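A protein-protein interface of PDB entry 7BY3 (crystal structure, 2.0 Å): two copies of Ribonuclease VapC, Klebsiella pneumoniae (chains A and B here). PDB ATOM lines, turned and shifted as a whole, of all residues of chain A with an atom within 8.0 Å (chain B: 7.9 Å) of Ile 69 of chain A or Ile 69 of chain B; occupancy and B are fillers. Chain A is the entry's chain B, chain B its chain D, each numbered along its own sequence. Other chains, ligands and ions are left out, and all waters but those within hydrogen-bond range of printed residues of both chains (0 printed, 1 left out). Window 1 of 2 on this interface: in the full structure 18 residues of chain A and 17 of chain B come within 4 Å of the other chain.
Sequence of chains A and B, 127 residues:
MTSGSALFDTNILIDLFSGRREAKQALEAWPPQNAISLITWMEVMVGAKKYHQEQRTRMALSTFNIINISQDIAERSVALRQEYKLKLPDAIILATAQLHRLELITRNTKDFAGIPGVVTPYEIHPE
Leu 38 of chain A touches Ser 70 of chain B, and with the chains exchanged Ser 70 of chain A touches Leu 38 of chain B. Leu 38 of chain A touches Ala 74 of chain B, but with the chains exchanged Ala 74 of chain A does not touch Leu 38 of chain B (4.03 Å). Asn 68 of chain A touches Ile 69 of chain B, but with the chains exchanged Ile 69 of chain A does not touch Asn 68 of chain B (4.04 Å). Ile 69 of chain B touches its own counterpart, Ile 69 of chain A. Of the 13 pairs that touch across the chains among the printed residues, 11 have their exchanged pair printed and touching as well.
Of the 20 printed residues of chain B, 7 touch a printed residue of chain A. Of the 20 printed residues of chain A, 8 touch a printed residue of chain B. Along chain A the printed residues that touch a printed residue of chain B span positions 38 to 92.
N of Leu 38 of chain A is in hydrogen-bond range of O of Ile 67 of chain A. The side-chain carboxylate (OE1) of Glu 75 of chain A sits at hydrogen-bond distance from the side-chain amide nitrogen (NE2) of Gln 71 of chain A (3.5 Å). The side-chain hydroxyl (OG1) of Thr 96 of chain A sits at hydrogen-bond distance from the backbone carbonyl oxygen (O) of Ile 92 of chain A (2.8 Å). The backbone NH of Leu 38 of chain B lies within hydrogen-bond range of the backbone carbonyl oxygen of Ile 67 of chain B (3.0 Å). The backbone NH of Ile 73 of chain B sits at hydrogen-bond distance from the side-chain hydroxyl of Ser 70 of chain B (3.3 Å). The backbone carbonyl oxygen of Ile 92 of chain B lies within hydrogen-bond range of the side-chain hydroxyl of Thr 96 of chain B, at 2.7 Å.
CD2 of Leu 38 of chain A touches O of Ile 69 of chain B, at 3.4 Å. Leu 38 of chain A touches Ser 70 of chain B. Ala 74 of chain B touches Leu 38 of chain A (CB to CD1, 3.8 Å). Ala 74 of chain B touches Met 42 of chain A. Ile 92 of chain B touches Met 42 of chain A. Ile 69 of chain B touches Asn 68 of chain A. O of Ile 69 of chain A touches CD2 of Leu 38 of chain B (3.4 Å). Ile 69 of chain A touches Ile 69 of chain B. Gln 71 of chain A touches Leu 38 of chain B. CG of Met 42 of chain B touches CB of Ala 74 of chain A (3.7 Å).
Of the printed residues of chain B, Leu 38 of chain A touches Ile 69 (3.4 Å), Ser 70 (3.3 Å), Gln 71 (3.7 Å) and Ala 74 (3.8 Å). Printed residues of chain B within 4 Å of Met 42 of chain A: Ala 74 and Ile 92. Ile 69 of chain A touches just these residues of chain B: Leu 38 (3.4 Å) and Ile 69 (3.9 Å). Of the printed residues of chain A, Ile 69 of chain B touches Leu 38 (3.4 Å), Asn 68 (3.98 Å) and Ile 69 (3.9 Å). Printed residues of chain A within 4 Å of Ala 74 of chain B: Leu 38 (3.8 Å) and Met 42 (3.7 Å). The nearest printed residue of chain A that does not touch Ala 74 of chain B is Asn 68 of chain A (7.0 Å).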
ATOM      1  N   SER A  37     -13.369  17.025 -11.757  1.00  0.00           N
ATOM      2  CA  SER A  37     -13.530  17.435 -13.145  1.00  0.00           C
ATOM      3  C   SER A  37     -12.463  16.782 -14.019  1.00  0.00           C
ATOM      4  O   SER A  37     -11.446  16.309 -13.516  1.00  0.00           O
ATOM      5  CB  SER A  37     -13.459  18.959 -13.271  1.00  0.00           C
ATOM      6  OG  SER A  37     -13.452  19.361 -14.630  1.00  0.00           O
ATOM      7  N   LEU A  38     -12.707  16.742 -15.324  1.00  0.00           N
ATOM      8  CA  LEU A  38     -11.696  16.290 -16.273  1.00  0.00           C
ATOM      9  C   LEU A  38     -10.489  17.229 -16.251  1.00  0.00           C
ATOM     10  O   LEU A  38      -9.358  16.810 -16.498  1.00  0.00           O
ATOM     11  CB  LEU A  38     -12.283  16.203 -17.685  1.00  0.00           C
ATOM     12  CG  LEU A  38     -11.498  15.408 -18.731  1.00  0.00           C
ATOM     13  CD1 LEU A  38     -11.059  14.052 -18.189  1.00  0.00           C
ATOM     14  CD2 LEU A  38     -12.327  15.241 -19.996  1.00  0.00           C
ATOM     15  N   ILE A  39     -10.743  18.499 -15.952  1.00  0.00           N
ATOM     16  CA  ILE A  39      -9.686  19.495 -15.809  1.00  0.00           C
ATOM     17  C   ILE A  39      -8.707  19.092 -14.714  1.00  0.00           C
ATOM     18  O   ILE A  39      -7.494  19.223 -14.870  1.00  0.00           O
ATOM     19  CB  ILE A  39     -10.267  20.887 -15.490  1.00  0.00           C
ATOM     20  CG1 ILE A  39     -11.034  21.426 -16.698  1.00  0.00           C
ATOM     21  CG2 ILE A  39      -9.165  21.853 -15.076  1.00  0.00           C
ATOM     22  CD1 ILE A  39     -11.219  22.919 -16.688  1.00  0.00           C
ATOM     23  N   THR A  40      -9.248  18.591 -13.610  1.00  0.00           N
ATOM     24  CA  THR A  40      -8.430  18.145 -12.490  1.00  0.00           C
ATOM     25  C   THR A  40      -7.646  16.886 -12.853  1.00  0.00           C
ATOM     26  O   THR A  40      -6.471  16.766 -12.513  1.00  0.00           O
ATOM     27  CB  THR A  40      -9.292  17.885 -11.238  1.00  0.00           C
ATOM     28  OG1 THR A  40      -9.833  19.125 -10.767  1.00  0.00           O
ATOM     29  CG2 THR A  40      -8.462  17.261 -10.132  1.00  0.00           C
ATOM     30  N   MET A  42      -6.485  15.983 -15.729  1.00  0.00           N
ATOM     31  CA  MET A  42      -5.360  16.354 -16.583  1.00  0.00           C
ATOM     32  C   MET A  42      -4.217  17.004 -15.807  1.00  0.00           C
ATOM     33  O   MET A  42      -3.051  16.672 -16.017  1.00  0.00           O
ATOM     34  CB  MET A  42      -5.826  17.296 -17.697  1.00  0.00           C
ATOM     35  CG  MET A  42      -6.733  16.642 -18.724  1.00  0.00           C
ATOM     36  SD  MET A  42      -7.068  17.708 -20.136  1.00  0.00           S
ATOM     37  CE  MET A  42      -8.626  18.436 -19.645  1.00  0.00           C
ATOM     38  N   ILE A  66     -15.526  10.919 -12.701  1.00  0.00           N
ATOM     39  CA  ILE A  66     -14.773  11.889 -13.480  1.00  0.00           C
ATOM     40  C   ILE A  66     -15.696  12.536 -14.493  1.00  0.00           C
ATOM     41  O   ILE A  66     -16.154  11.895 -15.435  1.00  0.00           O
ATOM     42  CB  ILE A  66     -13.568  11.243 -14.183  1.00  0.00           C
ATOM     43  CG1 ILE A  66     -12.648  10.593 -13.148  1.00  0.00           C
ATOM     44  CG2 ILE A  66     -12.804  12.281 -14.988  1.00  0.00           C
ATOM     45  CD1 ILE A  66     -11.494   9.824 -13.748  1.00  0.00           C
ATOM     46  N   ILE A  67     -15.968  13.818 -14.283  1.00  0.00           N
ATOM     47  CA  ILE A  67     -16.989  14.515 -15.047  1.00  0.00           C
ATOM     48  C   ILE A  67     -16.396  15.324 -16.198  1.00  0.00           C
ATOM     49  O   ILE A  67     -15.611  16.247 -15.988  1.00  0.00           O
ATOM     50  CB  ILE A  67     -17.811  15.440 -14.134  1.00  0.00           C
ATOM     51  CG1 ILE A  67     -18.273  14.671 -12.892  1.00  0.00           C
ATOM     52  CG2 ILE A  67     -18.994  16.020 -14.890  1.00  0.00           C
ATOM     53  CD1 ILE A  67     -19.142  15.471 -11.953  1.00  0.00           C
ATOM     54  N   ASN A  68     -16.784  14.960 -17.417  1.00  0.00           N
ATOM     55  CA  ASN A  68     -16.326  15.648 -18.616  1.00  0.00           C
ATOM     56  C   ASN A  68     -16.921  17.045 -18.734  1.00  0.00           C
ATOM     57  O   ASN A  68     -17.952  17.343 -18.131  1.00  0.00           O
ATOM     58  CB  ASN A  68     -16.678  14.839 -19.868  1.00  0.00           C
ATOM     59  CG  ASN A  68     -16.161  13.416 -19.814  1.00  0.00           C
ATOM     60  OD1 ASN A  68     -15.086  13.149 -19.279  1.00  0.00           O
ATOM     61  ND2 ASN A  68     -16.930  12.490 -20.377  1.00  0.00           N
ATOM     62  N   ILE A  69     -16.266  17.900 -19.514  1.00  0.00           N
ATOM     63  CA  ILE A  69     -16.802  19.222 -19.802  1.00  0.00           C
ATOM     64  C   ILE A  69     -17.632  19.165 -21.077  1.00  0.00           C
ATOM     65  O   ILE A  69     -17.111  18.917 -22.165  1.00  0.00           O
ATOM     66  CB  ILE A  69     -15.688  20.278 -19.955  1.00  0.00           C
ATOM     67  CG1 ILE A  69     -14.748  20.239 -18.750  1.00  0.00           C
ATOM     68  CG2 ILE A  69     -16.287  21.669 -20.123  1.00  0.00           C
ATOM     69  CD1 ILE A  69     -13.300  20.037 -19.121  1.00  0.00           C
ATOM     70  N   SER A  70     -18.930  19.394 -20.925  1.00  0.00           N
ATOM     71  CA  SER A  70     -19.854  19.397 -22.047  1.00  0.00           C
ATOM     72  C   SER A  70     -20.456  20.786 -22.222  1.00  0.00           C
ATOM     73  O   SER A  70     -20.065  21.727 -21.534  1.00  0.00           O
ATOM     74  CB  SER A  70     -20.951  18.354 -21.847  1.00  0.00           C
ATOM     75  OG  SER A  70     -21.705  18.641 -20.685  1.00  0.00           O
ATOM     76  N   GLN A  71     -21.401  20.906 -23.149  1.00  0.00           N
ATOM     77  CA  GLN A  71     -21.914  22.204 -23.575  1.00  0.00           C
ATOM     78  C   GLN A  71     -22.500  23.064 -22.449  1.00  0.00           C
ATOM     79  O   GLN A  71     -22.257  24.270 -22.406  1.00  0.00           O
ATOM     80  CB  GLN A  71     -22.967  22.011 -24.668  1.00  0.00           C
ATOM     81  CG  GLN A  71     -23.516  23.310 -25.229  1.00  0.00           C
ATOM     82  CD  GLN A  71     -22.437  24.178 -25.849  1.00  0.00           C
ATOM     83  OE1 GLN A  71     -21.736  23.757 -26.770  1.00  0.00           O
ATOM     84  NE2 GLN A  71     -22.296  25.397 -25.343  1.00  0.00           N
ATOM     85  N   ASP A  72     -23.269  22.470 -21.544  1.00  0.00           N
ATOM     86  CA  ASP A  72     -23.918  23.282 -20.517  1.00  0.00           C
ATOM     87  C   ASP A  72     -23.160  23.350 -19.190  1.00  0.00           C
ATOM     88  O   ASP A  72     -23.596  24.030 -18.262  1.00  0.00           O
ATOM     89  CB  ASP A  72     -25.350  22.804 -20.283  1.00  0.00           C
ATOM     90  CG  ASP A  72     -26.350  23.534 -21.165  1.00  0.00           C
ATOM     91  OD1 ASP A  72     -25.994  23.876 -22.314  1.00  0.00           O
ATOM     92  OD2 ASP A  72     -27.485  23.783 -20.706  1.00  0.00           O
ATOM     93  N   ILE A  73     -22.029  22.659 -19.095  1.00  0.00           N
ATOM     94  CA  ILE A  73     -21.057  22.992 -18.060  1.00  0.00           C
ATOM     95  C   ILE A  73     -20.338  24.235 -18.554  1.00  0.00           C
ATOM     96  O   ILE A  73     -20.092  25.176 -17.798  1.00  0.00           O
ATOM     97  CB  ILE A  73     -20.052  21.857 -17.783  1.00  0.00           C
ATOM     98  CG1 ILE A  73     -20.678  20.811 -16.862  1.00  0.00           C
ATOM     99  CG2 ILE A  73     -18.784  22.402 -17.144  1.00  0.00           C
ATOM    100  CD1 ILE A  73     -19.914  19.512 -16.811  1.00  0.00           C
ATOM    101  N   ALA A  74     -20.032  24.231 -19.846  1.00  0.00           N
ATOM    102  CA  ALA A  74     -19.442  25.380 -20.514  1.00  0.00           C
ATOM    103  C   ALA A  74     -20.364  26.587 -20.418  1.00  0.00           C
ATOM    104  O   ALA A  74     -19.905  27.712 -20.238  1.00  0.00           O
ATOM    105  CB  ALA A  74     -19.145  25.051 -21.967  1.00  0.00           C
ATOM    106  N   GLU A  75     -21.664  26.342 -20.536  1.00  0.00           N
ATOM    107  CA  GLU A  75     -22.660  27.404 -20.447  1.00  0.00           C
ATOM    108  C   GLU A  75     -22.624  28.080 -19.082  1.00  0.00           C
ATOM    109  O   GLU A  75     -22.570  29.305 -18.981  1.00  0.00           O
ATOM    110  CB  GLU A  75     -24.060  26.849 -20.713  1.00  0.00           C
ATOM    111  CG  GLU A  75     -25.010  27.848 -21.330  1.00  0.00           C
ATOM    112  CD  GLU A  75     -24.614  28.202 -22.744  1.00  0.00           C
ATOM    113  OE1 GLU A  75     -24.645  27.304 -23.608  1.00  0.00           O
ATOM    114  OE2 GLU A  75     -24.261  29.373 -22.988  1.00  0.00           O
ATOM    115  N   SER A  77     -20.192  27.831 -16.964  1.00  0.00           N
ATOM    116  CA  SER A  77     -18.826  28.285 -16.727  1.00  0.00           C
ATOM    117  C   SER A  77     -18.616  29.733 -17.156  1.00  0.00           C
ATOM    118  O   SER A  77     -17.977  30.509 -16.445  1.00  0.00           O
ATOM    119  CB  SER A  77     -17.834  27.379 -17.456  1.00  0.00           C
ATOM    120  OG  SER A  77     -17.915  26.052 -16.970  1.00  0.00           O
ATOM    121  N   ILE A  92     -15.065  26.486 -14.459  1.00  0.00           N
ATOM    122  CA  ILE A  92     -15.491  25.200 -15.000  1.00  0.00           C
ATOM    123  C   ILE A  92     -15.661  24.164 -13.890  1.00  0.00           C
ATOM    124  O   ILE A  92     -16.621  23.393 -13.890  1.00  0.00           O
ATOM    125  CB  ILE A  92     -14.492  24.683 -16.058  1.00  0.00           C
ATOM    126  CG1 ILE A  92     -14.486  25.612 -17.273  1.00  0.00           C
ATOM    127  CG2 ILE A  92     -14.846  23.271 -16.491  1.00  0.00           C
ATOM    128  CD1 ILE A  92     -13.384  25.326 -18.263  1.00  0.00           C
ATOM    129  N   ILE A  93     -14.735  24.163 -12.938  1.00  0.00           N
ATOM    130  CA  ILE A  93     -14.801  23.239 -11.812  1.00  0.00           C
ATOM    131  C   ILE A  93     -15.981  23.587 -10.902  1.00  0.00           C
ATOM    132  O   ILE A  93     -16.656  22.700 -10.378  1.00  0.00           O
ATOM    133  CB  ILE A  93     -13.478  23.243 -11.015  1.00  0.00           C
ATOM    134  CG1 ILE A  93     -12.399  22.496 -11.801  1.00  0.00           C
ATOM    135  CG2 ILE A  93     -13.654  22.589  -9.658  1.00  0.00           C
ATOM    136  CD1 ILE A  93     -11.021  22.591 -11.198  1.00  0.00           C
ATOM    137  N   ALA A  95     -18.693  25.184 -12.007  1.00  0.00           N
ATOM    138  CA  ALA A  95     -19.865  24.888 -12.828  1.00  0.00           C
ATOM    139  C   ALA A  95     -20.203  23.405 -12.779  1.00  0.00           C
ATOM    140  O   ALA A  95     -21.371  23.020 -12.744  1.00  0.00           O
ATOM    141  CB  ALA A  95     -19.632  25.327 -14.262  1.00  0.00           C
ATOM    142  N   THR A  96     -19.164  22.579 -12.780  1.00  0.00           N
ATOM    143  CA  THR A  96     -19.322  21.135 -12.703  1.00  0.00           C
ATOM    144  C   THR A  96     -19.972  20.731 -11.381  1.00  0.00           C
ATOM    145  O   THR A  96     -20.852  19.870 -11.349  1.00  0.00           O
ATOM    146  CB  THR A  96     -17.963  20.424 -12.861  1.00  0.00           C
ATOM    147  OG1 THR A  96     -17.439  20.687 -14.168  1.00  0.00           O
ATOM    148  CG2 THR A  96     -18.112  18.925 -12.677  1.00  0.00           C
ATOM    149  N   SER B  37     -12.529  24.065 -30.581  1.00  0.00           N
ATOM    150  CA  SER B  37     -12.601  23.332 -29.326  1.00  0.00           C
ATOM    151  C   SER B  37     -13.680  23.959 -28.452  1.00  0.00           C
ATOM    152  O   SER B  37     -13.998  25.136 -28.604  1.00  0.00           O
ATOM    153  CB  SER B  37     -11.249  23.339 -28.608  1.00  0.00           C
ATOM    154  OG  SER B  37     -11.350  22.769 -27.313  1.00  0.00           O
ATOM    155  N   LEU B  38     -14.251  23.171 -27.546  1.00  0.00           N
ATOM    156  CA  LEU B  38     -15.218  23.699 -26.591  1.00  0.00           C
ATOM    157  C   LEU B  38     -14.555  24.756 -25.715  1.00  0.00           C
ATOM    158  O   LEU B  38     -15.214  25.666 -25.210  1.00  0.00           O
ATOM    159  CB  LEU B  38     -15.802  22.579 -25.726  1.00  0.00           C
ATOM    160  CG  LEU B  38     -16.946  22.984 -24.792  1.00  0.00           C
ATOM    161  CD1 LEU B  38     -18.120  23.562 -25.572  1.00  0.00           C
ATOM    162  CD2 LEU B  38     -17.386  21.809 -23.934  1.00  0.00           C
ATOM    163  N   ILE B  39     -13.242  24.631 -25.545  1.00  0.00           N
ATOM    164  CA  ILE B  39     -12.472  25.620 -24.809  1.00  0.00           C
ATOM    165  C   ILE B  39     -12.541  26.966 -25.518  1.00  0.00           C
ATOM    166  O   ILE B  39     -12.824  27.981 -24.892  1.00  0.00           O
ATOM    167  CB  ILE B  39     -11.006  25.182 -24.639  1.00  0.00           C
ATOM    168  CG1 ILE B  39     -10.927  24.039 -23.623  1.00  0.00           C
ATOM    169  CG2 ILE B  39     -10.139  26.361 -24.212  1.00  0.00           C
ATOM    170  CD1 ILE B  39      -9.681  24.037 -22.775  1.00  0.00           C
ATOM    171  N   THR B  40     -12.315  26.959 -26.829  1.00  0.00           N
ATOM    172  CA  THR B  40     -12.402  28.175 -27.637  1.00  0.00           C
ATOM    173  C   THR B  40     -13.789  28.805 -27.547  1.00  0.00           C
ATOM    174  O   THR B  40     -13.919  30.024 -27.430  1.00  0.00           O
ATOM    175  CB  THR B  40     -12.059  27.890 -29.117  1.00  0.00           C
ATOM    176  OG1 THR B  40     -10.665  27.578 -29.232  1.00  0.00           O
ATOM    177  CG2 THR B  40     -12.375  29.096 -29.997  1.00  0.00           C
ATOM    178  N   MET B  42     -15.813  28.769 -25.088  1.00  0.00           N
ATOM    179  CA  MET B  42     -15.902  29.474 -23.811  1.00  0.00           C
ATOM    180  C   MET B  42     -15.108  30.780 -23.824  1.00  0.00           C
ATOM    181  O   MET B  42     -15.573  31.800 -23.315  1.00  0.00           O
ATOM    182  CB  MET B  42     -15.409  28.580 -22.670  1.00  0.00           C
ATOM    183  CG  MET B  42     -16.381  27.480 -22.278  1.00  0.00           C
ATOM    184  SD  MET B  42     -15.757  26.440 -20.945  1.00  0.00           S
ATOM    185  CE  MET B  42     -14.343  25.684 -21.737  1.00  0.00           C
ATOM    186  N   ILE B  66     -18.367  22.143 -32.785  1.00  0.00           N
ATOM    187  CA  ILE B  66     -17.841  22.409 -31.461  1.00  0.00           C
ATOM    188  C   ILE B  66     -17.507  21.079 -30.815  1.00  0.00           C
ATOM    189  O   ILE B  66     -18.391  20.296 -30.470  1.00  0.00           O
ATOM    190  CB  ILE B  66     -18.837  23.205 -30.607  1.00  0.00           C
ATOM    191  CG1 ILE B  66     -19.295  24.446 -31.375  1.00  0.00           C
ATOM    192  CG2 ILE B  66     -18.205  23.603 -29.285  1.00  0.00           C
ATOM    193  CD1 ILE B  66     -20.459  25.162 -30.746  1.00  0.00           C
ATOM    194  N   ILE B  67     -16.212  20.837 -30.659  1.00  0.00           N
ATOM    195  CA  ILE B  67     -15.724  19.534 -30.244  1.00  0.00           C
ATOM    196  C   ILE B  67     -15.458  19.506 -28.748  1.00  0.00           C
ATOM    197  O   ILE B  67     -14.597  20.224 -28.241  1.00  0.00           O
ATOM    198  CB  ILE B  67     -14.447  19.151 -31.009  1.00  0.00           C
ATOM    199  CG1 ILE B  67     -14.702  19.216 -32.518  1.00  0.00           C
ATOM    200  CG2 ILE B  67     -13.990  17.764 -30.602  1.00  0.00           C
ATOM    201  CD1 ILE B  67     -13.475  18.972 -33.364  1.00  0.00           C
ATOM    202  N   ASN B  68     -16.217  18.672 -28.048  1.00  0.00           N
ATOM    203  CA  ASN B  68     -16.119  18.571 -26.601  1.00  0.00           C
ATOM    204  C   ASN B  68     -14.827  17.908 -26.143  1.00  0.00           C
ATOM    205  O   ASN B  68     -14.171  17.197 -26.903  1.00  0.00           O
ATOM    206  CB  ASN B  68     -17.321  17.809 -26.047  1.00  0.00           C
ATOM    207  CG  ASN B  68     -18.615  18.587 -26.182  1.00  0.00           C
ATOM    208  OD1 ASN B  68     -18.616  19.818 -26.167  1.00  0.00           O
ATOM    209  ND2 ASN B  68     -19.725  17.872 -26.315  1.00  0.00           N
ATOM    210  N   ILE B  69     -14.476  18.144 -24.884  1.00  0.00           N
ATOM    211  CA  ILE B  69     -13.238  17.628 -24.326  1.00  0.00           C
ATOM    212  C   ILE B  69     -13.498  16.269 -23.693  1.00  0.00           C
ATOM    213  O   ILE B  69     -14.182  16.161 -22.676  1.00  0.00           O
ATOM    214  CB  ILE B  69     -12.653  18.595 -23.282  1.00  0.00           C
ATOM    215  CG1 ILE B  69     -12.666  20.023 -23.832  1.00  0.00           C
ATOM    216  CG2 ILE B  69     -11.246  18.173 -22.893  1.00  0.00           C
ATOM    217  CD1 ILE B  69     -13.109  21.064 -22.831  1.00  0.00           C
ATOM    218  N   SER B  70     -12.941  15.234 -24.309  1.00  0.00           N
ATOM    219  CA  SER B  70     -13.207  13.865 -23.901  1.00  0.00           C
ATOM    220  C   SER B  70     -12.065  13.298 -23.071  1.00  0.00           C
ATOM    221  O   SER B  70     -11.067  13.975 -22.830  1.00  0.00           O
ATOM    222  CB  SER B  70     -13.446  12.988 -25.130  1.00  0.00           C
ATOM    223  OG  SER B  70     -12.373  13.105 -26.046  1.00  0.00           O
ATOM    224  N   GLN B  71     -12.217  12.052 -22.638  1.00  0.00           N
ATOM    225  CA  GLN B  71     -11.188  11.388 -21.849  1.00  0.00           C
ATOM    226  C   GLN B  71      -9.939  11.133 -22.683  1.00  0.00           C
ATOM    227  O   GLN B  71      -8.817  11.291 -22.202  1.00  0.00           O
ATOM    228  CB  GLN B  71     -11.717  10.073 -21.273  1.00  0.00           C
ATOM    229  CG  GLN B  71     -10.677   9.251 -20.525  1.00  0.00           C
ATOM    230  CD  GLN B  71     -10.068   9.992 -19.349  1.00  0.00           C
ATOM    231  OE1 GLN B  71     -10.757  10.323 -18.384  1.00  0.00           O
ATOM    232  NE2 GLN B  71      -8.768  10.251 -19.422  1.00  0.00           N
ATOM    233  N   ASP B  72     -10.137  10.736 -23.935  1.00  0.00           N
ATOM    234  CA  ASP B  72      -9.019  10.424 -24.818  1.00  0.00           C
ATOM    235  C   ASP B  72      -8.372  11.683 -25.392  1.00  0.00           C
ATOM    236  O   ASP B  72      -7.196  11.666 -25.762  1.00  0.00           O
ATOM    237  CB  ASP B  72      -9.473   9.491 -25.942  1.00  0.00           C
ATOM    238  CG  ASP B  72      -9.872   8.118 -25.432  1.00  0.00           C
ATOM    239  OD1 ASP B  72      -9.269   7.650 -24.441  1.00  0.00           O
ATOM    240  OD2 ASP B  72     -10.781   7.501 -26.024  1.00  0.00           O
ATOM    241  N   ILE B  73      -9.137  12.768 -25.474  1.00  0.00           N
ATOM    242  CA  ILE B  73      -8.560  14.071 -25.788  1.00  0.00           C
ATOM    243  C   ILE B  73      -7.756  14.531 -24.574  1.00  0.00           C
ATOM    244  O   ILE B  73      -6.713  15.173 -24.708  1.00  0.00           O
ATOM    245  CB  ILE B  73      -9.646  15.115 -26.175  1.00  0.00           C
ATOM    246  CG1 ILE B  73      -9.915  15.071 -27.681  1.00  0.00           C
ATOM    247  CG2 ILE B  73      -9.232  16.524 -25.778  1.00  0.00           C
ATOM    248  CD1 ILE B  73     -10.824  16.177 -28.180  1.00  0.00           C
ATOM    249  N   ALA B  74      -8.230  14.163 -23.389  1.00  0.00           N
ATOM    250  CA  ALA B  74      -7.534  14.489 -22.151  1.00  0.00           C
ATOM    251  C   ALA B  74      -6.189  13.772 -22.062  1.00  0.00           C
ATOM    252  O   ALA B  74      -5.195  14.365 -21.654  1.00  0.00           O
ATOM    253  CB  ALA B  74      -8.396  14.149 -20.950  1.00  0.00           C
ATOM    254  N   GLU B  75      -6.165  12.499 -22.446  1.00  0.00           N
ATOM    255  CA  GLU B  75      -4.933  11.709 -22.425  1.00  0.00           C
ATOM    256  C   GLU B  75      -3.896  12.256 -23.406  1.00  0.00           C
ATOM    257  O   GLU B  75      -2.707  12.322 -23.094  1.00  0.00           O
ATOM    258  CB  GLU B  75      -5.237  10.242 -22.741  1.00  0.00           C
ATOM    259  CG  GLU B  75      -4.054   9.439 -23.283  1.00  0.00           C
ATOM    260  CD  GLU B  75      -3.046   9.053 -22.212  1.00  0.00           C
ATOM    261  OE1 GLU B  75      -2.192   9.893 -21.859  1.00  0.00           O
ATOM    262  OE2 GLU B  75      -3.099   7.902 -21.731  1.00  0.00           O
ATOM    263  N   SER B  77      -3.743  15.380 -24.589  1.00  0.00           N
ATOM    264  CA  SER B  77      -3.332  16.696 -24.110  1.00  0.00           C
ATOM    265  C   SER B  77      -2.230  16.578 -23.067  1.00  0.00           C
ATOM    266  O   SER B  77      -1.268  17.345 -23.082  1.00  0.00           O
ATOM    267  CB  SER B  77      -4.525  17.452 -23.525  1.00  0.00           C
ATOM    268  OG  SER B  77      -5.685  17.259 -24.311  1.00  0.00           O
ATOM    269  N   ILE B  92      -4.816  20.993 -25.184  1.00  0.00           N
ATOM    270  CA  ILE B  92      -6.162  20.486 -25.417  1.00  0.00           C
ATOM    271  C   ILE B  92      -6.623  20.781 -26.844  1.00  0.00           C
ATOM    272  O   ILE B  92      -7.190  19.922 -27.517  1.00  0.00           O
ATOM    273  CB  ILE B  92      -7.160  21.091 -24.405  1.00  0.00           C
ATOM    274  CG1 ILE B  92      -6.914  20.507 -23.013  1.00  0.00           C
ATOM    275  CG2 ILE B  92      -8.594  20.837 -24.834  1.00  0.00           C
ATOM    276  CD1 ILE B  92      -7.652  21.217 -21.908  1.00  0.00           C
ATOM    277  N   ILE B  93      -6.358  21.998 -27.300  1.00  0.00           N
ATOM    278  CA  ILE B  93      -6.725  22.418 -28.647  1.00  0.00           C
ATOM    279  C   ILE B  93      -5.918  21.663 -29.703  1.00  0.00           C
ATOM    280  O   ILE B  93      -6.460  21.242 -30.724  1.00  0.00           O
ATOM    281  CB  ILE B  93      -6.538  23.937 -28.813  1.00  0.00           C
ATOM    282  CG1 ILE B  93      -7.600  24.673 -27.996  1.00  0.00           C
ATOM    283  CG2 ILE B  93      -6.627  24.348 -30.271  1.00  0.00           C
ATOM    284  CD1 ILE B  93      -7.277  26.100 -27.738  1.00  0.00           C
ATOM    285  N   ALA B  95      -4.596  18.714 -29.201  1.00  0.00           N
ATOM    286  CA  ALA B  95      -5.075  17.339 -29.083  1.00  0.00           C
ATOM    287  C   ALA B  95      -6.360  17.134 -29.873  1.00  0.00           C
ATOM    288  O   ALA B  95      -6.543  16.107 -30.525  1.00  0.00           O
ATOM    289  CB  ALA B  95      -5.294  16.978 -27.623  1.00  0.00           C
ATOM    290  N   THR B  96      -7.245  18.120 -29.806  1.00  0.00           N
ATOM    291  CA  THR B  96      -8.510  18.075 -30.523  1.00  0.00           C
ATOM    292  C   THR B  96      -8.286  17.977 -32.027  1.00  0.00           C
ATOM    293  O   THR B  96      -8.968  17.224 -32.720  1.00  0.00           O
ATOM    294  CB  THR B  96      -9.364  19.315 -30.217  1.00  0.00           C
ATOM    295  OG1 THR B  96      -9.543  19.435 -28.802  1.00  0.00           O
ATOM    296  CG2 THR B  96     -10.717  19.204 -30.882  1.00  0.00           C
